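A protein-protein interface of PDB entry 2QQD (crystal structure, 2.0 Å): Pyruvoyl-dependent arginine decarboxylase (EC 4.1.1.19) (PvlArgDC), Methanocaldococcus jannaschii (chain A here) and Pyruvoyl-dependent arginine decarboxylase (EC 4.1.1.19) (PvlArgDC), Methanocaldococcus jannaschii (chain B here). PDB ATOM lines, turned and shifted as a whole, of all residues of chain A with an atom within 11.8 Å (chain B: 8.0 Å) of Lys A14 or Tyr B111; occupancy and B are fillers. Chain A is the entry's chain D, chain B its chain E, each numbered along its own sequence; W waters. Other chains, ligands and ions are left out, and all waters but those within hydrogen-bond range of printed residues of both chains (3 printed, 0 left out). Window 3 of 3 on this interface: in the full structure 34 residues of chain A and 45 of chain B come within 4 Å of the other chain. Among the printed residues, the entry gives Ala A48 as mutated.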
ATOM      1  N   ALA A   4       5.726 -13.603  20.473  1.00  0.00           N
ATOM      2  CA  ALA A   4       5.198 -13.337  21.846  1.00  0.00           C
ATOM      3  C   ALA A   4       3.665 -13.392  21.887  1.00  0.00           C
ATOM      4  O   ALA A   4       3.058 -13.355  22.958  1.00  0.00           O
ATOM      5  CB  ALA A   4       5.681 -11.978  22.324  1.00  0.00           C
ATOM      6  N   GLU A   5       3.043 -13.476  20.719  1.00  0.00           N
ATOM      7  CA  GLU A   5       1.587 -13.534  20.636  1.00  0.00           C
ATOM      8  C   GLU A   5       1.104 -14.920  20.241  1.00  0.00           C
ATOM      9  O   GLU A   5       1.842 -15.698  19.636  1.00  0.00           O
ATOM     10  CB  GLU A   5       1.073 -12.528  19.606  1.00  0.00           C
ATOM     11  CG  GLU A   5       1.102 -11.077  20.053  1.00  0.00           C
ATOM     12  CD  GLU A   5       0.747 -10.123  18.921  1.00  0.00           C
ATOM     13  OE1 GLU A   5      -0.104 -10.486  18.083  1.00  0.00           O
ATOM     14  OE2 GLU A   5       1.315  -9.009  18.872  1.00  0.00           O
ATOM     15  N   ILE A   6      -0.138 -15.231  20.588  1.00  0.00           N
ATOM     16  CA  ILE A   6      -0.714 -16.514  20.217  1.00  0.00           C
ATOM     17  C   ILE A   6      -2.230 -16.456  20.123  1.00  0.00           C
ATOM     18  O   ILE A   6      -2.894 -15.787  20.913  1.00  0.00           O
ATOM     19  CB  ILE A   6      -0.338 -17.640  21.216  1.00  0.00           C
ATOM     20  CG1 ILE A   6      -0.844 -18.987  20.681  1.00  0.00           C
ATOM     21  CG2 ILE A   6      -0.953 -17.364  22.589  1.00  0.00           C
ATOM     22  CD1 ILE A   6      -0.409 -20.192  21.500  1.00  0.00           C
ATOM     23  N   ASN A   7      -2.768 -17.141  19.123  1.00  0.00           N
ATOM     24  CA  ASN A   7      -4.208 -17.229  18.950  1.00  0.00           C
ATOM     25  C   ASN A   7      -4.490 -18.711  19.189  1.00  0.00           C
ATOM     26  O   ASN A   7      -4.297 -19.540  18.293  1.00  0.00           O
ATOM     27  CB  ASN A   7      -4.628 -16.840  17.527  1.00  0.00           C
ATOM     28  CG  ASN A   7      -6.130 -16.938  17.324  1.00  0.00           C
ATOM     29  OD1 ASN A   7      -6.831 -17.555  18.128  1.00  0.00           O
ATOM     30  ND2 ASN A   7      -6.629 -16.345  16.246  1.00  0.00           N
ATOM     31  N   PRO A   8      -4.928 -19.067  20.412  1.00  0.00           N
ATOM     32  CA  PRO A   8      -5.228 -20.461  20.764  1.00  0.00           C
ATOM     33  C   PRO A   8      -6.174 -21.176  19.790  1.00  0.00           C
ATOM     34  O   PRO A   8      -6.173 -22.402  19.707  1.00  0.00           O
ATOM     35  CB  PRO A   8      -5.828 -20.344  22.167  1.00  0.00           C
ATOM     36  CG  PRO A   8      -5.166 -19.124  22.718  1.00  0.00           C
ATOM     37  CD  PRO A   8      -5.205 -18.170  21.547  1.00  0.00           C
ATOM     38  N   LEU A   9      -6.985 -20.415  19.063  1.00  0.00           N
ATOM     39  CA  LEU A   9      -7.918 -20.997  18.100  1.00  0.00           C
ATOM     40  C   LEU A   9      -7.176 -21.523  16.869  1.00  0.00           C
ATOM     41  O   LEU A   9      -7.664 -22.414  16.172  1.00  0.00           O
ATOM     42  CB  LEU A   9      -8.948 -19.949  17.665  1.00  0.00           C
ATOM     43  CG  LEU A   9      -9.847 -19.378  18.766  1.00  0.00           C
ATOM     44  CD1 LEU A   9     -10.689 -18.238  18.213  1.00  0.00           C
ATOM     45  CD2 LEU A   9     -10.737 -20.480  19.321  1.00  0.00           C
ATOM     46  N   HIS A  10      -6.002 -20.960  16.600  1.00  0.00           N
ATOM     47  CA  HIS A  10      -5.207 -21.377  15.453  1.00  0.00           C
ATOM     48  C   HIS A  10      -4.053 -22.291  15.864  1.00  0.00           C
ATOM     49  O   HIS A  10      -3.769 -23.278  15.187  1.00  0.00           O
ATOM     50  CB  HIS A  10      -4.690 -20.145  14.710  1.00  0.00           C
ATOM     51  CG  HIS A  10      -5.767 -19.377  14.007  1.00  0.00           C
ATOM     52  ND1 HIS A  10      -5.552 -18.145  13.430  1.00  0.00           N
ATOM     53  CD2 HIS A  10      -7.067 -19.682  13.768  1.00  0.00           C
ATOM     54  CE1 HIS A  10      -6.670 -17.723  12.866  1.00  0.00           C
ATOM     55  NE2 HIS A  10      -7.604 -18.636  13.057  1.00  0.00           N
ATOM     56  N   ALA A  11      -3.400 -21.964  16.975  1.00  0.00           N
ATOM     57  CA  ALA A  11      -2.307 -22.778  17.485  1.00  0.00           C
ATOM     58  C   ALA A  11      -2.895 -23.877  18.385  1.00  0.00           C
ATOM     59  O   ALA A  11      -2.661 -23.897  19.596  1.00  0.00           O
ATOM     60  CB  ALA A  11      -1.335 -21.910  18.272  1.00  0.00           C
ATOM     61  N   TYR A  12      -3.658 -24.786  17.778  1.00  0.00           N
ATOM     62  CA  TYR A  12      -4.300 -25.886  18.497  1.00  0.00           C
ATOM     63  C   TYR A  12      -3.289 -26.880  19.083  1.00  0.00           C
ATOM     64  O   TYR A  12      -3.599 -27.609  20.026  1.00  0.00           O
ATOM     65  CB  TYR A  12      -5.256 -26.624  17.552  1.00  0.00           C
ATOM     66  CG  TYR A  12      -4.554 -27.355  16.431  1.00  0.00           C
ATOM     67  CD1 TYR A  12      -4.070 -28.649  16.619  1.00  0.00           C
ATOM     68  CD2 TYR A  12      -4.328 -26.737  15.194  1.00  0.00           C
ATOM     69  CE1 TYR A  12      -3.379 -29.315  15.614  1.00  0.00           C
ATOM     70  CE2 TYR A  12      -3.630 -27.399  14.181  1.00  0.00           C
ATOM     71  CZ  TYR A  12      -3.160 -28.688  14.403  1.00  0.00           C
ATOM     72  OH  TYR A  12      -2.471 -29.362  13.420  1.00  0.00           O
ATOM     73  N   PHE A  13      -2.083 -26.903  18.516  1.00  0.00           N
ATOM     74  CA  PHE A  13      -1.029 -27.814  18.958  1.00  0.00           C
ATOM     75  C   PHE A  13      -0.217 -27.268  20.136  1.00  0.00           C
ATOM     76  O   PHE A  13       0.624 -27.965  20.698  1.00  0.00           O
ATOM     77  CB  PHE A  13      -0.103 -28.127  17.774  1.00  0.00           C
ATOM     78  CG  PHE A  13       0.365 -26.899  17.039  1.00  0.00           C
ATOM     79  CD1 PHE A  13       1.422 -26.137  17.531  1.00  0.00           C
ATOM     80  CD2 PHE A  13      -0.286 -26.475  15.888  1.00  0.00           C
ATOM     81  CE1 PHE A  13       1.818 -24.971  16.889  1.00  0.00           C
ATOM     82  CE2 PHE A  13       0.103 -25.303  15.233  1.00  0.00           C
ATOM     83  CZ  PHE A  13       1.157 -24.550  15.736  1.00  0.00           C
ATOM     84  N   LYS A  14      -0.461 -26.018  20.512  1.00  0.00           N
ATOM     85  CA  LYS A  14       0.256 -25.424  21.634  1.00  0.00           C
ATOM     86  C   LYS A  14      -0.753 -25.235  22.761  1.00  0.00           C
ATOM     87  O   LYS A  14      -1.564 -24.312  22.735  1.00  0.00           O
ATOM     88  CB  LYS A  14       0.873 -24.079  21.230  1.00  0.00           C
ATOM     89  CG  LYS A  14       1.856 -23.506  22.244  1.00  0.00           C
ATOM     90  CD  LYS A  14       2.976 -24.506  22.551  1.00  0.00           C
ATOM     91  CE  LYS A  14       4.187 -23.834  23.196  1.00  0.00           C
ATOM     92  NZ  LYS A  14       3.905 -23.212  24.521  1.00  0.00           N
ATOM     93  N   LEU A  15      -0.708 -26.127  23.742  1.00  0.00           N
ATOM     94  CA  LEU A  15      -1.647 -26.063  24.854  1.00  0.00           C
ATOM     95  C   LEU A  15      -1.161 -25.231  26.025  1.00  0.00           C
ATOM     96  O   LEU A  15       0.036 -25.164  26.299  1.00  0.00           O
ATOM     97  CB  LEU A  15      -1.976 -27.477  25.342  1.00  0.00           C
ATOM     98  CG  LEU A  15      -2.856 -28.343  24.431  1.00  0.00           C
ATOM     99  CD1 LEU A  15      -2.240 -28.455  23.047  1.00  0.00           C
ATOM    100  CD2 LEU A  15      -3.012 -29.724  25.062  1.00  0.00           C
ATOM    101  N   PRO A  16      -2.096 -24.575  26.732  1.00  0.00           N
ATOM    102  CA  PRO A  16      -1.765 -23.742  27.894  1.00  0.00           C
ATOM    103  C   PRO A  16      -1.064 -24.626  28.924  1.00  0.00           C
ATOM    104  O   PRO A  16      -1.299 -25.839  28.958  1.00  0.00           O
ATOM    105  CB  PRO A  16      -3.135 -23.277  28.390  1.00  0.00           C
ATOM    106  CG  PRO A  16      -3.976 -23.275  27.126  1.00  0.00           C
ATOM    107  CD  PRO A  16      -3.545 -24.553  26.456  1.00  0.00           C
ATOM    108  N   ASN A  17      -0.207 -24.039  29.754  1.00  0.00           N
ATOM    109  CA  ASN A  17       0.475 -24.830  30.770  1.00  0.00           C
ATOM    110  C   ASN A  17       0.416 -24.193  32.151  1.00  0.00           C
ATOM    111  O   ASN A  17       1.066 -24.652  33.086  1.00  0.00           O
ATOM    112  CB  ASN A  17       1.923 -25.128  30.352  1.00  0.00           C
ATOM    113  CG  ASN A  17       2.768 -23.881  30.201  1.00  0.00           C
ATOM    114  OD1 ASN A  17       2.270 -22.810  29.870  1.00  0.00           O
ATOM    115  ND2 ASN A  17       4.069 -24.026  30.424  1.00  0.00           N
ATOM    116  N   THR A  18      -0.382 -23.136  32.276  1.00  0.00           N
ATOM    117  CA  THR A  18      -0.568 -22.472  33.553  1.00  0.00           C
ATOM    118  C   THR A  18      -2.055 -22.141  33.701  1.00  0.00           C
ATOM    119  O   THR A  18      -2.787 -22.028  32.714  1.00  0.00           O
ATOM    120  CB  THR A  18       0.259 -21.163  33.669  1.00  0.00           C
ATOM    121  OG1 THR A  18      -0.419 -20.092  33.009  1.00  0.00           O
ATOM    122  CG2 THR A  18       1.632 -21.337  33.031  1.00  0.00           C
ATOM    123  N   VAL A  19      -2.502 -22.030  34.941  1.00  0.00           N
ATOM    124  CA  VAL A  19      -3.879 -21.682  35.223  1.00  0.00           C
ATOM    125  C   VAL A  19      -3.812 -20.747  36.415  1.00  0.00           C
ATOM    126  O   VAL A  19      -3.023 -20.952  37.334  1.00  0.00           O
ATOM    127  CB  VAL A  19      -4.745 -22.933  35.545  1.00  0.00           C
ATOM    128  CG1 VAL A  19      -4.075 -23.784  36.590  1.00  0.00           C
ATOM    129  CG2 VAL A  19      -6.132 -22.499  36.020  1.00  0.00           C
ATOM    130  N   SER A  20      -4.615 -19.694  36.373  1.00  0.00           N
ATOM    131  CA  SER A  20      -4.637 -18.719  37.445  1.00  0.00           C
ATOM    132  C   SER A  20      -6.080 -18.493  37.867  1.00  0.00           C
ATOM    133  O   SER A  20      -6.953 -18.308  37.023  1.00  0.00           O
ATOM    134  CB  SER A  20      -4.019 -17.399  36.969  1.00  0.00           C
ATOM    135  OG  SER A  20      -2.667 -17.572  36.554  1.00  0.00           O
ATOM    136  N   ILE A  44      -8.595  -9.328  34.587  1.00  0.00           N
ATOM    137  CA  ILE A  44      -8.621  -9.817  33.207  1.00  0.00           C
ATOM    138  C   ILE A  44      -9.622  -9.041  32.366  1.00  0.00           C
ATOM    139  O   ILE A  44     -10.250  -9.589  31.461  1.00  0.00           O
ATOM    140  CB  ILE A  44      -8.986 -11.321  33.119  1.00  0.00           C
ATOM    141  CG1 ILE A  44     -10.296 -11.588  33.864  1.00  0.00           C
ATOM    142  CG2 ILE A  44      -7.845 -12.172  33.666  1.00  0.00           C
ATOM    143  CD1 ILE A  44     -10.785 -13.010  33.724  1.00  0.00           C
ATOM    144  N   VAL A  47      -8.302  -8.074  28.297  1.00  0.00           N
ATOM    145  CA  VAL A  47      -7.987  -9.179  27.396  1.00  0.00           C
ATOM    146  C   VAL A  47      -9.300  -9.724  26.846  1.00  0.00           C
ATOM    147  O   VAL A  47     -10.373  -9.490  27.408  1.00  0.00           O
ATOM    148  CB  VAL A  47      -7.256 -10.369  28.107  1.00  0.00           C
ATOM    149  CG1 VAL A  47      -5.814  -9.998  28.440  1.00  0.00           C
ATOM    150  CG2 VAL A  47      -8.018 -10.769  29.367  1.00  0.00           C
ATOM    151  N   ALA A  48      -9.207 -10.447  25.736  1.00  0.00           N
ATOM    152  CA  ALA A  48     -10.369 -11.059  25.121  1.00  0.00           C
ATOM    153  C   ALA A  48     -10.459 -12.484  25.651  1.00  0.00           C
ATOM    154  O   ALA A  48      -9.570 -13.311  25.405  1.00  0.00           O
ATOM    155  CB  ALA A  48     -10.228 -11.068  23.608  1.00  0.00           C
ATOM    156  N   LEU A  49     -11.531 -12.768  26.382  1.00  0.00           N
ATOM    157  CA  LEU A  49     -11.722 -14.090  26.942  1.00  0.00           C
ATOM    158  C   LEU A  49     -12.393 -15.069  25.991  1.00  0.00           C
ATOM    159  O   LEU A  49     -13.459 -14.787  25.448  1.00  0.00           O
ATOM    160  CB  LEU A  49     -12.561 -14.003  28.214  1.00  0.00           C
ATOM    161  CG  LEU A  49     -12.069 -13.101  29.354  1.00  0.00           C
ATOM    162  CD1 LEU A  49     -13.055 -13.207  30.513  1.00  0.00           C
ATOM    163  CD2 LEU A  49     -10.684 -13.516  29.810  1.00  0.00           C
ATOM    164  N   ILE A  50     -11.758 -16.216  25.769  1.00  0.00           N
ATOM    165  CA  ILE A  50     -12.367 -17.251  24.945  1.00  0.00           C
ATOM    166  C   ILE A  50     -12.899 -18.221  25.997  1.00  0.00           C
ATOM    167  O   ILE A  50     -12.128 -18.913  26.664  1.00  0.00           O
ATOM    168  CB  ILE A  50     -11.348 -17.984  24.055  1.00  0.00           C
ATOM    169  CG1 ILE A  50     -10.745 -17.008  23.041  1.00  0.00           C
ATOM    170  CG2 ILE A  50     -12.046 -19.134  23.306  1.00  0.00           C
ATOM    171  CD1 ILE A  50      -9.584 -17.591  22.247  1.00  0.00           C
ATOM    172  N   ARG A  51     -14.215 -18.256  26.166  1.00  0.00           N
ATOM    173  CA  ARG A  51     -14.792 -19.126  27.177  1.00  0.00           C
ATOM    174  C   ARG A  51     -14.682 -20.616  26.852  1.00  0.00           C
ATOM    175  O   ARG A  51     -15.069 -21.067  25.770  1.00  0.00           O
ATOM    176  CB  ARG A  51     -16.259 -18.754  27.423  1.00  0.00           C
ATOM    177  CG  ARG A  51     -16.832 -19.393  28.692  1.00  0.00           C
ATOM    178  CD  ARG A  51     -18.266 -18.945  28.971  1.00  0.00           C
ATOM    179  NE  ARG A  51     -18.676 -19.316  30.324  1.00  0.00           N
ATOM    180  CZ  ARG A  51     -19.838 -18.969  30.878  1.00  0.00           C
ATOM    181  NH1 ARG A  51     -20.718 -18.246  30.196  1.00  0.00           N
ATOM    182  NH2 ARG A  51     -20.110 -19.320  32.129  1.00  0.00           N
ATOM    183  N   ILE A  52     -14.129 -21.378  27.789  1.00  0.00           N
ATOM    184  CA  ILE A  52     -14.014 -22.809  27.599  1.00  0.00           C
ATOM    185  C   ILE A  52     -14.986 -23.502  28.529  1.00  0.00           C
ATOM    186  O   ILE A  52     -15.246 -23.033  29.636  1.00  0.00           O
ATOM    187  CB  ILE A  52     -12.587 -23.317  27.854  1.00  0.00           C
ATOM    188  CG1 ILE A  52     -12.110 -22.903  29.248  1.00  0.00           C
ATOM    189  CG2 ILE A  52     -11.665 -22.791  26.752  1.00  0.00           C
ATOM    190  CD1 ILE A  52     -10.777 -23.520  29.633  1.00  0.00           C
ATOM    191  N   PRO B   3      -5.199 -28.695  31.102  1.00  0.00           N
ATOM    192  CA  PRO B   3      -4.182 -29.642  30.630  1.00  0.00           C
ATOM    193  C   PRO B   3      -3.368 -30.276  31.749  1.00  0.00           C
ATOM    194  O   PRO B   3      -3.082 -29.639  32.759  1.00  0.00           O
ATOM    195  CB  PRO B   3      -3.305 -28.789  29.711  1.00  0.00           C
ATOM    196  CG  PRO B   3      -4.236 -27.700  29.254  1.00  0.00           C
ATOM    197  CD  PRO B   3      -4.979 -27.363  30.516  1.00  0.00           C
ATOM    198  N   VAL B   9      -0.634 -20.686  38.999  1.00  0.00           N
ATOM    199  CA  VAL B   9       0.263 -19.564  39.240  1.00  0.00           C
ATOM    200  C   VAL B   9      -0.532 -18.279  39.391  1.00  0.00           C
ATOM    201  O   VAL B   9      -1.680 -18.204  38.962  1.00  0.00           O
ATOM    202  CB  VAL B   9       1.237 -19.353  38.059  1.00  0.00           C
ATOM    203  CG1 VAL B   9       1.997 -20.634  37.777  1.00  0.00           C
ATOM    204  CG2 VAL B   9       0.460 -18.902  36.810  1.00  0.00           C
ATOM    205  N   PRO B  12      -0.511 -13.837  35.590  1.00  0.00           N
ATOM    206  CA  PRO B  12       0.652 -13.160  35.002  1.00  0.00           C
ATOM    207  C   PRO B  12       0.257 -11.816  34.405  1.00  0.00           C
ATOM    208  O   PRO B  12      -0.924 -11.461  34.375  1.00  0.00           O
ATOM    209  CB  PRO B  12       1.118 -14.126  33.905  1.00  0.00           C
ATOM    210  CG  PRO B  12       0.323 -15.407  34.139  1.00  0.00           C
ATOM    211  CD  PRO B  12      -0.969 -14.923  34.713  1.00  0.00           C
ATOM    212  N   LEU B  14      -0.710 -10.096  31.605  1.00  0.00           N
ATOM    213  CA  LEU B  14      -1.248 -10.453  30.301  1.00  0.00           C
ATOM    214  C   LEU B  14      -1.136  -9.330  29.285  1.00  0.00           C
ATOM    215  O   LEU B  14      -1.449  -8.180  29.575  1.00  0.00           O
ATOM    216  CB  LEU B  14      -2.722 -10.860  30.433  1.00  0.00           C
ATOM    217  CG  LEU B  14      -3.074 -12.059  31.321  1.00  0.00           C
ATOM    218  CD1 LEU B  14      -4.589 -12.170  31.443  1.00  0.00           C
ATOM    219  CD2 LEU B  14      -2.489 -13.337  30.737  1.00  0.00           C
ATOM    220  N   ALA B  18      -4.899  -9.738  24.556  1.00  0.00           N
ATOM    221  CA  ALA B  18      -4.573 -11.135  24.270  1.00  0.00           C
ATOM    222  C   ALA B  18      -5.850 -11.982  24.290  1.00  0.00           C
ATOM    223  O   ALA B  18      -6.847 -11.604  24.912  1.00  0.00           O
ATOM    224  CB  ALA B  18      -3.580 -11.669  25.307  1.00  0.00           C
ATOM    225  N   LEU B  19      -5.829 -13.113  23.590  1.00  0.00           N
ATOM    226  CA  LEU B  19      -6.974 -14.016  23.581  1.00  0.00           C
ATOM    227  C   LEU B  19      -6.644 -15.039  24.655  1.00  0.00           C
ATOM    228  O   LEU B  19      -5.678 -15.793  24.521  1.00  0.00           O
ATOM    229  CB  LEU B  19      -7.134 -14.680  22.208  1.00  0.00           C
ATOM    230  CG  LEU B  19      -7.727 -13.779  21.122  1.00  0.00           C
ATOM    231  CD1 LEU B  19      -7.386 -14.324  19.736  1.00  0.00           C
ATOM    232  CD2 LEU B  19      -9.249 -13.687  21.319  1.00  0.00           C
ATOM    233  N   VAL B  20      -7.438 -15.048  25.725  1.00  0.00           N
ATOM    234  CA  VAL B  20      -7.189 -15.927  26.861  1.00  0.00           C
ATOM    235  C   VAL B  20      -8.275 -16.985  27.096  1.00  0.00           C
ATOM    236  O   VAL B  20      -9.418 -16.646  27.397  1.00  0.00           O
ATOM    237  CB  VAL B  20      -7.051 -15.069  28.157  1.00  0.00           C
ATOM    238  CG1 VAL B  20      -6.622 -15.933  29.329  1.00  0.00           C
ATOM    239  CG2 VAL B  20      -6.067 -13.921  27.927  1.00  0.00           C
ATOM    240  N   PRO B  21      -7.935 -18.279  26.944  1.00  0.00           N
ATOM    241  CA  PRO B  21      -8.919 -19.348  27.164  1.00  0.00           C
ATOM    242  C   PRO B  21      -9.273 -19.278  28.646  1.00  0.00           C
ATOM    243  O   PRO B  21      -8.392 -19.340  29.503  1.00  0.00           O
ATOM    244  CB  PRO B  21      -8.141 -20.617  26.816  1.00  0.00           C
ATOM    245  CG  PRO B  21      -7.097 -20.125  25.845  1.00  0.00           C
ATOM    246  CD  PRO B  21      -6.655 -18.838  26.481  1.00  0.00           C
ATOM    247  N   ALA B 108      -8.128 -18.615  34.499  1.00  0.00           N
ATOM    248  CA  ALA B 108      -7.555 -18.182  33.234  1.00  0.00           C
ATOM    249  C   ALA B 108      -6.360 -19.062  32.884  1.00  0.00           C
ATOM    250  O   ALA B 108      -5.432 -19.210  33.674  1.00  0.00           O
ATOM    251  CB  ALA B 108      -7.129 -16.724  33.333  1.00  0.00           C
ATOM    252  N   LEU B 109      -6.404 -19.662  31.705  1.00  0.00           N
ATOM    253  CA  LEU B 109      -5.323 -20.513  31.259  1.00  0.00           C
ATOM    254  C   LEU B 109      -4.330 -19.646  30.499  1.00  0.00           C
ATOM    255  O   LEU B 109      -4.722 -18.758  29.741  1.00  0.00           O
ATOM    256  CB  LEU B 109      -5.856 -21.610  30.336  1.00  0.00           C
ATOM    257  CG  LEU B 109      -6.956 -22.527  30.879  1.00  0.00           C
ATOM    258  CD1 LEU B 109      -7.091 -23.736  29.968  1.00  0.00           C
ATOM    259  CD2 LEU B 109      -6.606 -22.974  32.286  1.00  0.00           C
ATOM    260  N   TRP B 110      -3.044 -19.896  30.694  1.00  0.00           N
ATOM    261  CA  TRP B 110      -2.047 -19.112  29.990  1.00  0.00           C
ATOM    262  C   TRP B 110      -0.816 -19.949  29.677  1.00  0.00           C
ATOM    263  O   TRP B 110      -0.849 -21.175  29.761  1.00  0.00           O
ATOM    264  CB  TRP B 110      -1.662 -17.865  30.799  1.00  0.00           C
ATOM    265  CG  TRP B 110      -1.033 -16.790  29.942  1.00  0.00           C
ATOM    266  CD1 TRP B 110       0.094 -16.062  30.224  1.00  0.00           C
ATOM    267  CD2 TRP B 110      -1.485 -16.344  28.655  1.00  0.00           C
ATOM    268  NE1 TRP B 110       0.373 -15.195  29.186  1.00  0.00           N
ATOM    269  CE2 TRP B 110      -0.577 -15.348  28.212  1.00  0.00           C
ATOM    270  CE3 TRP B 110      -2.566 -16.689  27.831  1.00  0.00           C
ATOM    271  CZ2 TRP B 110      -0.721 -14.697  26.981  1.00  0.00           C
ATOM    272  CZ3 TRP B 110      -2.706 -16.040  26.605  1.00  0.00           C
ATOM    273  CH2 TRP B 110      -1.787 -15.056  26.194  1.00  0.00           C
ATOM    274  N   TYR B 111       0.271 -19.281  29.318  1.00  0.00           N
ATOM    275  CA  TYR B 111       1.492 -19.977  28.936  1.00  0.00           C
ATOM    276  C   TYR B 111       2.698 -19.517  29.727  1.00  0.00           C
ATOM    277  O   TYR B 111       2.755 -18.386  30.206  1.00  0.00           O
ATOM    278  CB  TYR B 111       1.732 -19.771  27.446  1.00  0.00           C
ATOM    279  CG  TYR B 111       0.500 -20.058  26.618  1.00  0.00           C
ATOM    280  CD1 TYR B 111       0.286 -21.314  26.058  1.00  0.00           C
ATOM    281  CD2 TYR B 111      -0.484 -19.087  26.449  1.00  0.00           C
ATOM    282  CE1 TYR B 111      -0.880 -21.597  25.348  1.00  0.00           C
ATOM    283  CE2 TYR B 111      -1.654 -19.358  25.748  1.00  0.00           C
ATOM    284  CZ  TYR B 111      -1.848 -20.614  25.200  1.00  0.00           C
ATOM    285  OH  TYR B 111      -3.025 -20.883  24.525  1.00  0.00           O
ATOM    286  N   LYS B 112       3.663 -20.417  29.850  1.00  0.00           N
ATOM    287  CA  LYS B 112       4.884 -20.164  30.595  1.00  0.00           C
ATOM    288  C   LYS B 112       5.987 -21.047  30.013  1.00  0.00           C
ATOM    289  O   LYS B 112       7.150 -20.653  29.970  1.00  0.00           O
ATOM    290  CB  LYS B 112       4.642 -20.508  32.069  1.00  0.00           C
ATOM    291  CG  LYS B 112       5.870 -20.575  32.945  1.00  0.00           C
ATOM    292  CD  LYS B 112       5.506 -21.110  34.327  1.00  0.00           C
ATOM    293  CE  LYS B 112       6.739 -21.230  35.214  1.00  0.00           C
ATOM    294  NZ  LYS B 112       7.804 -22.053  34.562  1.00  0.00           N
HETATM  295  O   HOH W   1      -2.569 -18.581  33.933  1.00  0.00           O
HETATM  296  O   HOH W   2      -3.531 -14.637  23.197  1.00  0.00           O
HETATM  297  O   HOH W   3       1.365 -18.060  32.764  1.00  0.00           O
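Of chain B, only Tyr B111 (3.8 Å) comes within 4 Å of Lys A14.
Of chain A, only Ile A6, Pro A8, Lys A14, Leu A15, Pro A16, Asn A17 and Thr A18 come within 4 Å of Tyr B111.
Of chain A, only Pro A8 (3.8 Å) and Ile A50 (3.3 Å) come within 4 Å of Pro B21.
Of chain A, only Pro A16 (3.3 Å), Asn A17 (2.9 Å) and Thr A18 (2.9 Å) come within 4 Å of Trp B110.
Of chain A, only Asn A17 and Thr A18 come within 4 Å of Lys B112.
Printed residues of chain B within 4 Å of Pro A16: Pro B3, Leu B109, Trp B110 and Tyr B111.
Of the printed residues of chain B, Val A19 touches Val B9, Ala B108 and Leu B109.
Of the printed residues of chain B, Leu A15 touches Tyr B111 (3.7 Å).
The nearest residue of chain B that does not touch Lys A14 is Lys B112 (6.0 Å).
The nearest residue of chain A that does not touch Tyr B111 is Ala A11 (5.8 Å).
N of Lys B112 lies within hydrogen-bond range of OD1 of Asn A17 (2.8 Å).
N of Ile A50 is in hydrogen-bond range of O of Val B20, at 2.9 Å.
The backbone NH (N) of Ala A48 sits at hydrogen-bond distance from the backbone carbonyl oxygen (O) of Ala B18 (2.8 Å).
The side-chain hydroxyl of Ser A20 is in hydrogen-bond range of the backbone carbonyl oxygen of Val B9 (2.7 Å).
O of Ala A48 sits at hydrogen-bond distance from N of Val B20.
O of Ser A20 is in hydrogen-bond range of N of Ala B108 (2.8 Å).
The backbone carbonyl oxygen (O) of Val A19 sits at hydrogen-bond distance from the backbone NH (N) of Val B9.
The backbone carbonyl oxygen (O) of Trp B110 sits at hydrogen-bond distance from the backbone NH (N) of Asn A17 (2.9 Å).
O of Thr A18 lies within hydrogen-bond range of N of Trp B110 (2.9 Å).
Hydrophobic or aromatic side chains of chain B that line the printed part of chain A: Pro B3, Val B9, Pro B12, Leu B14, Leu B19, Val B20, Pro B21, Leu B109, Trp B110 and Tyr B111.
Of the 24 printed residues of chain A, 16 touch a printed residue of chain B.
Printed residues of chain A that touch a printed residue of chain B: Ile A6, Asn A7, Pro A8, Lys A14, Leu A15, Pro A16, Asn A17, Thr A18, Val A19, Ser A20, Ile A44, Val A47, Ala A48, Leu A49, Ile A50 and Ile A52.
Along chain A the printed residues that touch a printed residue of chain B span positions 6 to 52.
OD1 of Asn A7 sits at hydrogen-bond distance from N of Leu A9 (3.0 Å).
The backbone carbonyl oxygen of Pro B21 lies within hydrogen-bond range of the backbone NH of Leu B109 (3.0 Å).
Water W2 lies within hydrogen-bond range of the backbone carbonyl oxygen of Ile A6 (2.6 Å) and the backbone carbonyl oxygen of Leu B19 (2.8 Å).
Water W3 lies within hydrogen-bond range of the side-chain hydroxyl of Thr A18 and the backbone carbonyl oxygen of Tyr B111.
Water W1 lies within hydrogen-bond range of the side-chain hydroxyl (OG1) of Thr A18, the side-chain hydroxyl (OG) of Ser A20 and the backbone carbonyl oxygen (O) of Ala B108.
Among the printed residues, merely in contact across the chains: Ile A6 with Tyr B111 (3.8 Å), Asn A7 with Leu B19 (3.7 Å), Pro A8 with Leu B19 (3.8 Å), Pro A8 with Pro B21 (3.8 Å), Pro A8 with Tyr B111 (3.3 Å), Lys A14 with Tyr B111 (3.8 Å), Leu A15 with Tyr B111 (3.7 Å), Pro A16 with Pro B3 (3.5 Å), Pro A16 with Leu B109 (3.7 Å), Pro A16 with Trp B110 (3.3 Å), Pro A16 with Tyr B111 (3.4 Å), Asn A17 with Tyr B111 (3.1 Å), Thr A18 with Val B9 (3.9 Å), Thr A18 with Ala B108 (3.98 Å), Thr A18 with Leu B109 (3.3 Å), Thr A18 with Tyr B111 (3.8 Å), Thr A18 with Lys B112 (3.3 Å), Val A19 with Ala B108 (3.3 Å), Val A19 with Leu B109 (3.8 Å), Ser A20 with Pro B12 (3.6 Å), Ile A44 with Leu B14 (3.9 Å), Val A47 with Leu B14 (3.8 Å), Val A47 with Ala B18 (3.4 Å), Val A47 with Val B20 (3.8 Å), Ala A48 with Leu B19 (3.3 Å), Leu A49 with Val B20 (3.5 Å), Ile A50 with Leu B19 (3.8 Å), Ile A50 with Pro B21 (3.3 Å) and Ile A52 with Leu B109 (3.7 Å).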
